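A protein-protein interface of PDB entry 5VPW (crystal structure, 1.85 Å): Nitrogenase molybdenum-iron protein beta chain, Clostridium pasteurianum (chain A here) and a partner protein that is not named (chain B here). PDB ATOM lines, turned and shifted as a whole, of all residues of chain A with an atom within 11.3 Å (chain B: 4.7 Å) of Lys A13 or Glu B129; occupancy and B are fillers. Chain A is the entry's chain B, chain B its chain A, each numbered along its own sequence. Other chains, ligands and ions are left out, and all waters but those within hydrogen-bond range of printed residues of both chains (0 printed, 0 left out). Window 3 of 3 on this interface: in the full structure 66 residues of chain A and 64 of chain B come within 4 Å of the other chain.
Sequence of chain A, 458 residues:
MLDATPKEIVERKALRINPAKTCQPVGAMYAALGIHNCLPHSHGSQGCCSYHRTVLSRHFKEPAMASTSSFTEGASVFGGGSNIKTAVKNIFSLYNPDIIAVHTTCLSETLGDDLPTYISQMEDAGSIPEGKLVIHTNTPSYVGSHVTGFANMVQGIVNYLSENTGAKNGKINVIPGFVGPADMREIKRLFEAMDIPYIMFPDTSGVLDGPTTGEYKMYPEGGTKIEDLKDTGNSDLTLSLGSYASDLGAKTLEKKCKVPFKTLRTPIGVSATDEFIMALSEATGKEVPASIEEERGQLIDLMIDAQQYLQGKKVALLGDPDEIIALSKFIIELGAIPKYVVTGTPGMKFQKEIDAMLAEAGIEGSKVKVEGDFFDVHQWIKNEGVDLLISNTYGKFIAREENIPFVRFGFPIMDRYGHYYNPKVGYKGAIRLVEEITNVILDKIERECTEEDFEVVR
CG of Arg A12 touches OE1 of Glu B129, 3.7 Å away. Arg A12 touches Met B133. Lys B122 touches Ala A14. Asp B125 touches Ala A14 (CB to CB, 3.5 Å). CB of Ala A14 touches N of Ala B126 (3.5 Å). Leu A15 touches Ala B126 (CD1 to O, 3.97 Å). Leu A15 touches Ala B130. Met B133 touches Phe A375 (CE to CZ, 3.5 Å).
The backbone NH of Lys A13 lies within hydrogen-bond range of the side-chain carboxylate of Glu B129, 2.9 Å away. The backbone NH of Ala A14 is in hydrogen-bond range of the side-chain carboxylate of Glu B129, 3.0 Å away. The side-chain carboxylate (OE1) of Glu B129 lies within hydrogen-bond range of the backbone NH (N) of Leu A15.
Pro A6 touches none of the printed residues of chain B. Printed residues of chain B within 4 Å of Arg A12: Glu B129 (3.7 Å) and Met B133 (3.7 Å). Lys A13 touches one residue of chain B. Of the printed residues of chain B, Ala A14 touches Lys B122, Asp B125, Ala B126 and Glu B129. Of the printed residues of chain B, Leu A15 touches Ala B126, Glu B129 and Ala B130. Gly A372 touches none of the printed residues of chain B. Printed residues of chain B within 4 Å of Phe A375: Met B133. Of the printed residues of chain A, Lys B122 touches Ala A14 (3.5 Å). Ala B126 touches just these residues of chain A: Ala A14 and Leu A15. No residue of chain A comes within 4 Å of His B128. Of chain A, only Arg A12, Lys A13, Ala A14 and Leu A15 come within 4 Å of Glu B129. Ala B130 touches just one residue of chain A: Leu A15. Met B133 touches just these residues of chain A: Arg A12 and Phe A375. The nearest residue of chain A that does not touch Glu B129 is Glu A11 (4.1 Å).
Hydrophobic or aromatic side chains of chain B that line the printed part of chain A: Ala B130 and Met B133. Printed residues of chain A that touch a printed residue of chain B: Arg A12, Lys A13, Ala A14, Leu A15 and Phe A375. Hydrophobic or aromatic side chains of chain A within 4 Å of the printed part of chain B: Ala A14, Leu A15 and Phe A375.
The guanidinium group (NH1) of Arg A12 is in hydrogen-bond range of the backbone carbonyl oxygen (O) of Leu A15 (2.9 Å). The guanidinium group (NH1) of Arg A12 lies within salt-bridge range of the side-chain carboxylate (OD2) of Asp A373 (3.0 Å). The guanidinium group (NH2) of Arg A12 is in salt-bridge range of the side-chain carboxylate (OD1) of Asp A376. The backbone NH of Phe A375 lies close to the side-chain carboxylate of Asp A373.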
ATOM      1  N   ALA A   4     -27.857 -10.280 -18.129  1.00  0.00           N
ATOM      2  CA  ALA A   4     -26.764 -10.997 -17.465  1.00  0.00           C
ATOM      3  C   ALA A   4     -26.649 -10.724 -15.939  1.00  0.00           C
ATOM      4  O   ALA A   4     -25.935 -11.445 -15.229  1.00  0.00           O
ATOM      5  CB  ALA A   4     -25.453 -10.690 -18.181  1.00  0.00           C
ATOM      6  N   THR A   5     -27.362  -9.705 -15.444  1.00  0.00           N
ATOM      7  CA  THR A   5     -27.282  -9.277 -14.027  1.00  0.00           C
ATOM      8  C   THR A   5     -27.992 -10.256 -13.079  1.00  0.00           C
ATOM      9  O   THR A   5     -29.226 -10.207 -12.953  1.00  0.00           O
ATOM     10  CB  THR A   5     -27.904  -7.860 -13.805  1.00  0.00           C
ATOM     11  OG1 THR A   5     -27.394  -6.926 -14.770  1.00  0.00           O
ATOM     12  CG2 THR A   5     -27.619  -7.337 -12.373  1.00  0.00           C
ATOM     13  N   PRO A   6     -27.222 -11.134 -12.390  1.00  0.00           N
ATOM     14  CA  PRO A   6     -27.891 -12.037 -11.444  1.00  0.00           C
ATOM     15  C   PRO A   6     -28.629 -11.277 -10.320  1.00  0.00           C
ATOM     16  O   PRO A   6     -28.272 -10.133  -9.994  1.00  0.00           O
ATOM     17  CB  PRO A   6     -26.734 -12.891 -10.883  1.00  0.00           C
ATOM     18  CG  PRO A   6     -25.592 -12.705 -11.833  1.00  0.00           C
ATOM     19  CD  PRO A   6     -25.756 -11.318 -12.375  1.00  0.00           C
ATOM     20  N   GLU A   8     -28.975 -12.795  -7.213  1.00  0.00           N
ATOM     21  CA  GLU A   8     -28.164 -13.187  -6.051  1.00  0.00           C
ATOM     22  C   GLU A   8     -26.770 -12.553  -6.108  1.00  0.00           C
ATOM     23  O   GLU A   8     -26.033 -12.723  -7.090  1.00  0.00           O
ATOM     24  CB  GLU A   8     -28.056 -14.713  -5.948  1.00  0.00           C
ATOM     25  CG  GLU A   8     -29.359 -15.386  -5.541  1.00  0.00           C
ATOM     26  CD  GLU A   8     -29.301 -16.896  -5.655  1.00  0.00           C
ATOM     27  OE1 GLU A   8     -28.286 -17.484  -5.226  1.00  0.00           O
ATOM     28  OE2 GLU A   8     -30.272 -17.493  -6.173  1.00  0.00           O
ATOM     29  N   ILE A   9     -26.430 -11.827  -5.042  1.00  0.00           N
ATOM     30  CA  ILE A   9     -25.208 -11.033  -4.978  1.00  0.00           C
ATOM     31  C   ILE A   9     -24.002 -11.882  -4.534  1.00  0.00           C
ATOM     32  O   ILE A   9     -23.955 -12.350  -3.391  1.00  0.00           O
ATOM     33  CB  ILE A   9     -25.406  -9.815  -4.031  1.00  0.00           C
ATOM     34  CG1 ILE A   9     -26.544  -8.921  -4.557  1.00  0.00           C
ATOM     35  CG2 ILE A   9     -24.109  -9.015  -3.874  1.00  0.00           C
ATOM     36  CD1 ILE A   9     -26.927  -7.774  -3.645  1.00  0.00           C
ATOM     37  N   VAL A  10     -23.051 -12.083  -5.453  1.00  0.00           N
ATOM     38  CA  VAL A  10     -21.753 -12.711  -5.159  1.00  0.00           C
ATOM     39  C   VAL A  10     -20.674 -11.625  -4.998  1.00  0.00           C
ATOM     40  O   VAL A  10     -20.678 -10.629  -5.734  1.00  0.00           O
ATOM     41  CB  VAL A  10     -21.330 -13.692  -6.284  1.00  0.00           C
ATOM     42  CG1 VAL A  10     -19.921 -14.230  -6.035  1.00  0.00           C
ATOM     43  CG2 VAL A  10     -22.353 -14.823  -6.415  1.00  0.00           C
ATOM     44  N   GLU A  11     -19.752 -11.847  -4.053  1.00  0.00           N
ATOM     45  CA  GLU A  11     -18.717 -10.870  -3.660  1.00  0.00           C
ATOM     46  C   GLU A  11     -17.920 -10.389  -4.877  1.00  0.00           C
ATOM     47  O   GLU A  11     -17.525 -11.186  -5.719  1.00  0.00           O
ATOM     48  CB  GLU A  11     -17.744 -11.470  -2.627  1.00  0.00           C
ATOM     49  CG  GLU A  11     -18.340 -12.469  -1.638  1.00  0.00           C
ATOM     50  CD  GLU A  11     -19.576 -11.949  -0.914  1.00  0.00           C
ATOM     51  OE1 GLU A  11     -19.750 -10.711  -0.811  1.00  0.00           O
ATOM     52  OE2 GLU A  11     -20.375 -12.787  -0.439  1.00  0.00           O
ATOM     53  N   ARG A  12     -17.694  -9.085  -4.982  1.00  0.00           N
ATOM     54  CA  ARG A  12     -17.074  -8.530  -6.186  1.00  0.00           C
ATOM     55  C   ARG A  12     -16.040  -7.471  -5.821  1.00  0.00           C
ATOM     56  O   ARG A  12     -16.406  -6.417  -5.359  1.00  0.00           O
ATOM     57  CB  ARG A  12     -18.159  -7.958  -7.104  1.00  0.00           C
ATOM     58  CG  ARG A  12     -17.663  -7.591  -8.489  1.00  0.00           C
ATOM     59  CD  ARG A  12     -18.798  -7.417  -9.483  1.00  0.00           C
ATOM     60  NE  ARG A  12     -19.838  -6.511  -8.999  1.00  0.00           N
ATOM     61  CZ  ARG A  12     -19.891  -5.202  -9.219  1.00  0.00           C
ATOM     62  NH1 ARG A  12     -18.968  -4.570  -9.942  1.00  0.00           N
ATOM     63  NH2 ARG A  12     -20.927  -4.512  -8.749  1.00  0.00           N
ATOM     64  N   LYS A  13     -14.750  -7.762  -6.005  1.00  0.00           N
ATOM     65  CA  LYS A  13     -13.684  -6.881  -5.508  1.00  0.00           C
ATOM     66  C   LYS A  13     -12.712  -6.404  -6.577  1.00  0.00           C
ATOM     67  O   LYS A  13     -11.822  -5.626  -6.290  1.00  0.00           O
ATOM     68  CB  LYS A  13     -12.859  -7.605  -4.431  1.00  0.00           C
ATOM     69  CG  LYS A  13     -13.660  -8.030  -3.219  1.00  0.00           C
ATOM     70  CD  LYS A  13     -12.754  -8.341  -2.032  1.00  0.00           C
ATOM     71  CE  LYS A  13     -13.575  -8.643  -0.785  1.00  0.00           C
ATOM     72  NZ  LYS A  13     -14.513  -9.776  -1.040  1.00  0.00           N
ATOM     73  N   ALA A  14     -12.830  -6.879  -7.804  1.00  0.00           N
ATOM     74  CA  ALA A  14     -11.872  -6.439  -8.814  1.00  0.00           C
ATOM     75  C   ALA A  14     -12.552  -5.934 -10.075  1.00  0.00           C
ATOM     76  O   ALA A  14     -12.031  -5.038 -10.725  1.00  0.00           O
ATOM     77  CB  ALA A  14     -10.919  -7.578  -9.160  1.00  0.00           C
ATOM     78  N   LEU A  15     -13.669  -6.551 -10.431  1.00  0.00           N
ATOM     79  CA  LEU A  15     -14.323  -6.268 -11.695  1.00  0.00           C
ATOM     80  C   LEU A  15     -15.300  -5.123 -11.462  1.00  0.00           C
ATOM     81  O   LEU A  15     -16.289  -5.286 -10.743  1.00  0.00           O
ATOM     82  CB  LEU A  15     -15.049  -7.518 -12.192  1.00  0.00           C
ATOM     83  CG  LEU A  15     -15.740  -7.382 -13.540  1.00  0.00           C
ATOM     84  CD1 LEU A  15     -14.734  -7.251 -14.669  1.00  0.00           C
ATOM     85  CD2 LEU A  15     -16.649  -8.592 -13.742  1.00  0.00           C
ATOM     86  N   ARG A  16     -14.995  -3.974 -12.047  1.00  0.00           N
ATOM     87  CA  ARG A  16     -15.856  -2.811 -12.039  1.00  0.00           C
ATOM     88  C   ARG A  16     -16.808  -2.864 -13.249  1.00  0.00           C
ATOM     89  O   ARG A  16     -16.372  -3.082 -14.380  1.00  0.00           O
ATOM     90  CB  ARG A  16     -14.961  -1.563 -12.092  1.00  0.00           C
ATOM     91  CG  ARG A  16     -15.675  -0.231 -12.244  1.00  0.00           C
ATOM     92  CD  ARG A  16     -16.549   0.033 -11.058  1.00  0.00           C
ATOM     93  NE  ARG A  16     -15.761   0.237  -9.855  1.00  0.00           N
ATOM     94  CZ  ARG A  16     -16.214   0.018  -8.627  1.00  0.00           C
ATOM     95  NH1 ARG A  16     -17.437  -0.457  -8.439  1.00  0.00           N
ATOM     96  NH2 ARG A  16     -15.440   0.237  -7.581  1.00  0.00           N
ATOM     97  N   ILE A  17     -18.106  -2.727 -12.994  1.00  0.00           N
ATOM     98  CA  ILE A  17     -19.132  -2.825 -14.025  1.00  0.00           C
ATOM     99  C   ILE A  17     -20.001  -1.589 -13.985  1.00  0.00           C
ATOM    100  O   ILE A  17     -20.596  -1.280 -12.953  1.00  0.00           O
ATOM    101  CB  ILE A  17     -20.042  -4.069 -13.846  1.00  0.00           C
ATOM    102  CG1 ILE A  17     -19.202  -5.316 -13.564  1.00  0.00           C
ATOM    103  CG2 ILE A  17     -20.955  -4.199 -15.063  1.00  0.00           C
ATOM    104  CD1 ILE A  17     -20.018  -6.579 -13.240  1.00  0.00           C
ATOM    105  N   LYS A 369     -23.271   3.382  -0.389  1.00  0.00           N
ATOM    106  CA  LYS A 369     -21.982   2.843  -0.852  1.00  0.00           C
ATOM    107  C   LYS A 369     -21.122   3.846  -1.582  1.00  0.00           C
ATOM    108  O   LYS A 369     -21.549   4.444  -2.562  1.00  0.00           O
ATOM    109  CB  LYS A 369     -22.196   1.626  -1.737  1.00  0.00           C
ATOM    110  CG  LYS A 369     -20.910   0.898  -2.074  1.00  0.00           C
ATOM    111  CD  LYS A 369     -21.173  -0.486  -2.617  1.00  0.00           C
ATOM    112  CE  LYS A 369     -19.847  -1.205  -2.876  1.00  0.00           C
ATOM    113  NZ  LYS A 369     -20.039  -2.446  -3.668  1.00  0.00           N
ATOM    114  N   VAL A 370     -19.884   3.981  -1.114  1.00  0.00           N
ATOM    115  CA  VAL A 370     -18.878   4.782  -1.746  1.00  0.00           C
ATOM    116  C   VAL A 370     -18.078   3.840  -2.647  1.00  0.00           C
ATOM    117  O   VAL A 370     -17.719   2.753  -2.230  1.00  0.00           O
ATOM    118  CB  VAL A 370     -17.979   5.435  -0.675  1.00  0.00           C
ATOM    119  CG1 VAL A 370     -16.804   6.157  -1.313  1.00  0.00           C
ATOM    120  CG2 VAL A 370     -18.795   6.384   0.192  1.00  0.00           C
ATOM    121  N   GLU A 371     -17.814   4.262  -3.881  1.00  0.00           N
ATOM    122  CA  GLU A 371     -17.200   3.417  -4.908  1.00  0.00           C
ATOM    123  C   GLU A 371     -18.084   2.226  -5.247  1.00  0.00           C
ATOM    124  O   GLU A 371     -17.614   1.130  -5.483  1.00  0.00           O
ATOM    125  CB  GLU A 371     -15.782   2.973  -4.511  1.00  0.00           C
ATOM    126  CG  GLU A 371     -14.778   4.123  -4.425  1.00  0.00           C
ATOM    127  CD  GLU A 371     -13.322   3.657  -4.223  1.00  0.00           C
ATOM    128  OE1 GLU A 371     -12.625   3.330  -5.219  1.00  0.00           O
ATOM    129  OE2 GLU A 371     -12.860   3.633  -3.063  1.00  0.00           O
ATOM    130  N   GLY A 372     -19.392   2.443  -5.252  1.00  0.00           N
ATOM    131  CA  GLY A 372     -20.303   1.455  -5.779  1.00  0.00           C
ATOM    132  C   GLY A 372     -20.553   1.866  -7.226  1.00  0.00           C
ATOM    133  O   GLY A 372     -20.084   2.942  -7.674  1.00  0.00           O
ATOM    134  N   ASP A 373     -21.270   1.009  -7.948  1.00  0.00           N
ATOM    135  CA  ASP A 373     -21.530   1.198  -9.369  1.00  0.00           C
ATOM    136  C   ASP A 373     -23.000   0.883  -9.750  1.00  0.00           C
ATOM    137  O   ASP A 373     -23.782   0.530  -8.886  1.00  0.00           O
ATOM    138  CB  ASP A 373     -20.511   0.431 -10.233  1.00  0.00           C
ATOM    139  CG  ASP A 373     -20.436  -1.070  -9.939  1.00  0.00           C
ATOM    140  OD1 ASP A 373     -21.460  -1.716  -9.643  1.00  0.00           O
ATOM    141  OD2 ASP A 373     -19.327  -1.634 -10.090  1.00  0.00           O
ATOM    142  N   PHE A 375     -24.263  -1.497 -11.454  1.00  0.00           N
ATOM    143  CA  PHE A 375     -24.538  -2.933 -11.298  1.00  0.00           C
ATOM    144  C   PHE A 375     -24.914  -3.285  -9.824  1.00  0.00           C
ATOM    145  O   PHE A 375     -25.801  -4.111  -9.587  1.00  0.00           O
ATOM    146  CB  PHE A 375     -23.308  -3.729 -11.772  1.00  0.00           C
ATOM    147  CG  PHE A 375     -23.547  -5.200 -11.945  1.00  0.00           C
ATOM    148  CD1 PHE A 375     -23.363  -6.060 -10.889  1.00  0.00           C
ATOM    149  CD2 PHE A 375     -23.942  -5.714 -13.157  1.00  0.00           C
ATOM    150  CE1 PHE A 375     -23.607  -7.429 -11.035  1.00  0.00           C
ATOM    151  CE2 PHE A 375     -24.158  -7.073 -13.316  1.00  0.00           C
ATOM    152  CZ  PHE A 375     -23.998  -7.927 -12.252  1.00  0.00           C
ATOM    153  N   ASP A 376     -24.239  -2.667  -8.864  1.00  0.00           N
ATOM    154  CA  ASP A 376     -24.558  -2.809  -7.428  1.00  0.00           C
ATOM    155  C   ASP A 376     -26.032  -2.445  -7.214  1.00  0.00           C
ATOM    156  O   ASP A 376     -26.818  -3.236  -6.676  1.00  0.00           O
ATOM    157  CB  ASP A 376     -23.722  -1.866  -6.568  1.00  0.00           C
ATOM    158  CG  ASP A 376     -22.289  -2.375  -6.294  1.00  0.00           C
ATOM    159  OD1 ASP A 376     -22.074  -3.571  -6.099  1.00  0.00           O
ATOM    160  OD2 ASP A 376     -21.369  -1.537  -6.276  1.00  0.00           O
ATOM    161  N   GLN A 379     -28.632  -4.858  -8.768  1.00  0.00           N
ATOM    162  CA  GLN A 379     -28.744  -6.078  -7.964  1.00  0.00           C
ATOM    163  C   GLN A 379     -29.542  -5.798  -6.687  1.00  0.00           C
ATOM    164  O   GLN A 379     -30.403  -6.600  -6.297  1.00  0.00           O
ATOM    165  CB  GLN A 379     -27.352  -6.631  -7.631  1.00  0.00           C
ATOM    166  CG  GLN A 379     -26.624  -7.252  -8.805  1.00  0.00           C
ATOM    167  CD  GLN A 379     -25.455  -8.090  -8.333  1.00  0.00           C
ATOM    168  OE1 GLN A 379     -24.525  -7.572  -7.720  1.00  0.00           O
ATOM    169  NE2 GLN A 379     -25.518  -9.399  -8.580  1.00  0.00           N
ATOM    170  N   LYS B 122      -5.013  -7.698  -9.641  1.00  0.00           N
ATOM    171  CA  LYS B 122      -6.368  -7.203  -9.845  1.00  0.00           C
ATOM    172  C   LYS B 122      -6.963  -7.691 -11.162  1.00  0.00           C
ATOM    173  O   LYS B 122      -8.137  -8.055 -11.215  1.00  0.00           O
ATOM    174  CB  LYS B 122      -6.392  -5.678  -9.771  1.00  0.00           C
ATOM    175  CG  LYS B 122      -7.811  -5.132  -9.677  1.00  0.00           C
ATOM    176  CD  LYS B 122      -7.854  -3.713  -9.151  1.00  0.00           C
ATOM    177  CE  LYS B 122      -9.276  -3.290  -8.789  1.00  0.00           C
ATOM    178  NZ  LYS B 122      -9.361  -1.796  -8.867  1.00  0.00           N
ATOM    179  N   ASP B 125      -7.963 -11.282 -10.768  1.00  0.00           N
ATOM    180  CA  ASP B 125      -9.183 -11.440 -10.000  1.00  0.00           C
ATOM    181  C   ASP B 125     -10.372 -11.034 -10.841  1.00  0.00           C
ATOM    182  O   ASP B 125     -11.439 -11.666 -10.765  1.00  0.00           O
ATOM    183  CB  ASP B 125      -9.157 -10.619  -8.703  1.00  0.00           C
ATOM    184  CG  ASP B 125      -8.235 -11.239  -7.634  1.00  0.00           C
ATOM    185  OD1 ASP B 125      -7.875 -12.422  -7.757  1.00  0.00           O
ATOM    186  OD2 ASP B 125      -7.860 -10.527  -6.704  1.00  0.00           O
ATOM    187  N   ALA B 126     -10.200  -9.980 -11.642  1.00  0.00           N
ATOM    188  CA  ALA B 126     -11.316  -9.504 -12.498  1.00  0.00           C
ATOM    189  C   ALA B 126     -11.727 -10.510 -13.560  1.00  0.00           C
ATOM    190  O   ALA B 126     -12.925 -10.684 -13.823  1.00  0.00           O
ATOM    191  CB  ALA B 126     -10.995  -8.162 -13.117  1.00  0.00           C
ATOM    192  N   ILE B 127     -10.752 -11.187 -14.170  1.00  0.00           N
ATOM    193  CA  ILE B 127     -11.057 -12.211 -15.161  1.00  0.00           C
ATOM    194  C   ILE B 127     -11.873 -13.351 -14.521  1.00  0.00           C
ATOM    195  O   ILE B 127     -12.846 -13.853 -15.101  1.00  0.00           O
ATOM    196  CB  ILE B 127      -9.779 -12.792 -15.772  1.00  0.00           C
ATOM    197  CG1 ILE B 127      -9.069 -11.726 -16.626  1.00  0.00           C
ATOM    198  CG2 ILE B 127     -10.093 -14.016 -16.657  1.00  0.00           C
ATOM    199  CD1 ILE B 127      -7.640 -12.055 -16.976  1.00  0.00           C
ATOM    200  N   HIS B 128     -11.476 -13.765 -13.313  1.00  0.00           N
ATOM    201  CA  HIS B 128     -12.171 -14.869 -12.648  1.00  0.00           C
ATOM    202  C   HIS B 128     -13.574 -14.440 -12.235  1.00  0.00           C
ATOM    203  O   HIS B 128     -14.517 -15.231 -12.306  1.00  0.00           O
ATOM    204  CB  HIS B 128     -11.386 -15.374 -11.412  1.00  0.00           C
ATOM    205  CG  HIS B 128     -10.237 -16.257 -11.775  1.00  0.00           C
ATOM    206  ND1 HIS B 128     -10.379 -17.614 -11.983  1.00  0.00           N
ATOM    207  CD2 HIS B 128      -8.943 -15.969 -12.037  1.00  0.00           C
ATOM    208  CE1 HIS B 128      -9.215 -18.122 -12.346  1.00  0.00           C
ATOM    209  NE2 HIS B 128      -8.327 -17.147 -12.379  1.00  0.00           N
ATOM    210  N   GLU B 129     -13.710 -13.206 -11.774  1.00  0.00           N
ATOM    211  CA  GLU B 129     -15.035 -12.687 -11.391  1.00  0.00           C
ATOM    212  C   GLU B 129     -15.962 -12.644 -12.615  1.00  0.00           C
ATOM    213  O   GLU B 129     -17.135 -13.038 -12.536  1.00  0.00           O
ATOM    214  CB  GLU B 129     -14.906 -11.327 -10.708  1.00  0.00           C
ATOM    215  CG  GLU B 129     -14.475 -11.438  -9.262  1.00  0.00           C
ATOM    216  CD  GLU B 129     -14.241 -10.099  -8.569  1.00  0.00           C
ATOM    217  OE1 GLU B 129     -14.370  -9.014  -9.197  1.00  0.00           O
ATOM    218  OE2 GLU B 129     -13.920 -10.131  -7.369  1.00  0.00           O
ATOM    219  N   ALA B 130     -15.430 -12.225 -13.768  1.00  0.00           N
ATOM    220  CA  ALA B 130     -16.252 -12.149 -14.959  1.00  0.00           C
ATOM    221  C   ALA B 130     -16.728 -13.535 -15.376  1.00  0.00           C
ATOM    222  O   ALA B 130     -17.887 -13.714 -15.793  1.00  0.00           O
ATOM    223  CB  ALA B 130     -15.496 -11.496 -16.090  1.00  0.00           C
ATOM    224  N   TYR B 131     -15.819 -14.497 -15.282  1.00  0.00           N
ATOM    225  CA  TYR B 131     -16.108 -15.854 -15.703  1.00  0.00           C
ATOM    226  C   TYR B 131     -17.185 -16.440 -14.818  1.00  0.00           C
ATOM    227  O   TYR B 131     -18.175 -16.984 -15.313  1.00  0.00           O
ATOM    228  CB  TYR B 131     -14.860 -16.742 -15.628  1.00  0.00           C
ATOM    229  CG  TYR B 131     -15.211 -18.159 -15.927  1.00  0.00           C
ATOM    230  CD1 TYR B 131     -15.530 -18.559 -17.226  1.00  0.00           C
ATOM    231  CD2 TYR B 131     -15.323 -19.094 -14.903  1.00  0.00           C
ATOM    232  CE1 TYR B 131     -15.903 -19.867 -17.498  1.00  0.00           C
ATOM    233  CE2 TYR B 131     -15.691 -20.404 -15.169  1.00  0.00           C
ATOM    234  CZ  TYR B 131     -15.972 -20.781 -16.461  1.00  0.00           C
ATOM    235  OH  TYR B 131     -16.357 -22.071 -16.731  1.00  0.00           O
ATOM    236  N   GLU B 132     -16.983 -16.354 -13.509  1.00  0.00           N
ATOM    237  CA  GLU B 132     -17.935 -16.928 -12.556  1.00  0.00           C
ATOM    238  C   GLU B 132     -19.326 -16.247 -12.614  1.00  0.00           C
ATOM    239  O   GLU B 132     -20.333 -16.903 -12.467  1.00  0.00           O
ATOM    240  CB  GLU B 132     -17.372 -16.874 -11.131  1.00  0.00           C
ATOM    241  CG  GLU B 132     -16.122 -17.732 -10.928  1.00  0.00           C
ATOM    242  CD  GLU B 132     -16.333 -19.238 -11.218  1.00  0.00           C
ATOM    243  OE1 GLU B 132     -15.311 -19.963 -11.335  1.00  0.00           O
ATOM    244  OE2 GLU B 132     -17.493 -19.716 -11.344  1.00  0.00           O
ATOM    245  N   MET B 133     -19.371 -14.946 -12.866  1.00  0.00           N
ATOM    246  CA  MET B 133     -20.649 -14.245 -12.945  1.00  0.00           C
ATOM    247  C   MET B 133     -21.405 -14.394 -14.244  1.00  0.00           C
ATOM    248  O   MET B 133     -22.622 -14.359 -14.231  1.00  0.00           O
ATOM    249  CB  MET B 133     -20.469 -12.754 -12.691  1.00  0.00           C
ATOM    250  CG  MET B 133     -19.895 -12.395 -11.330  1.00  0.00           C
ATOM    251  SD  MET B 133     -19.675 -10.598 -11.166  1.00  0.00           S
ATOM    252  CE  MET B 133     -21.372 -10.126 -11.466  1.00  0.00           C
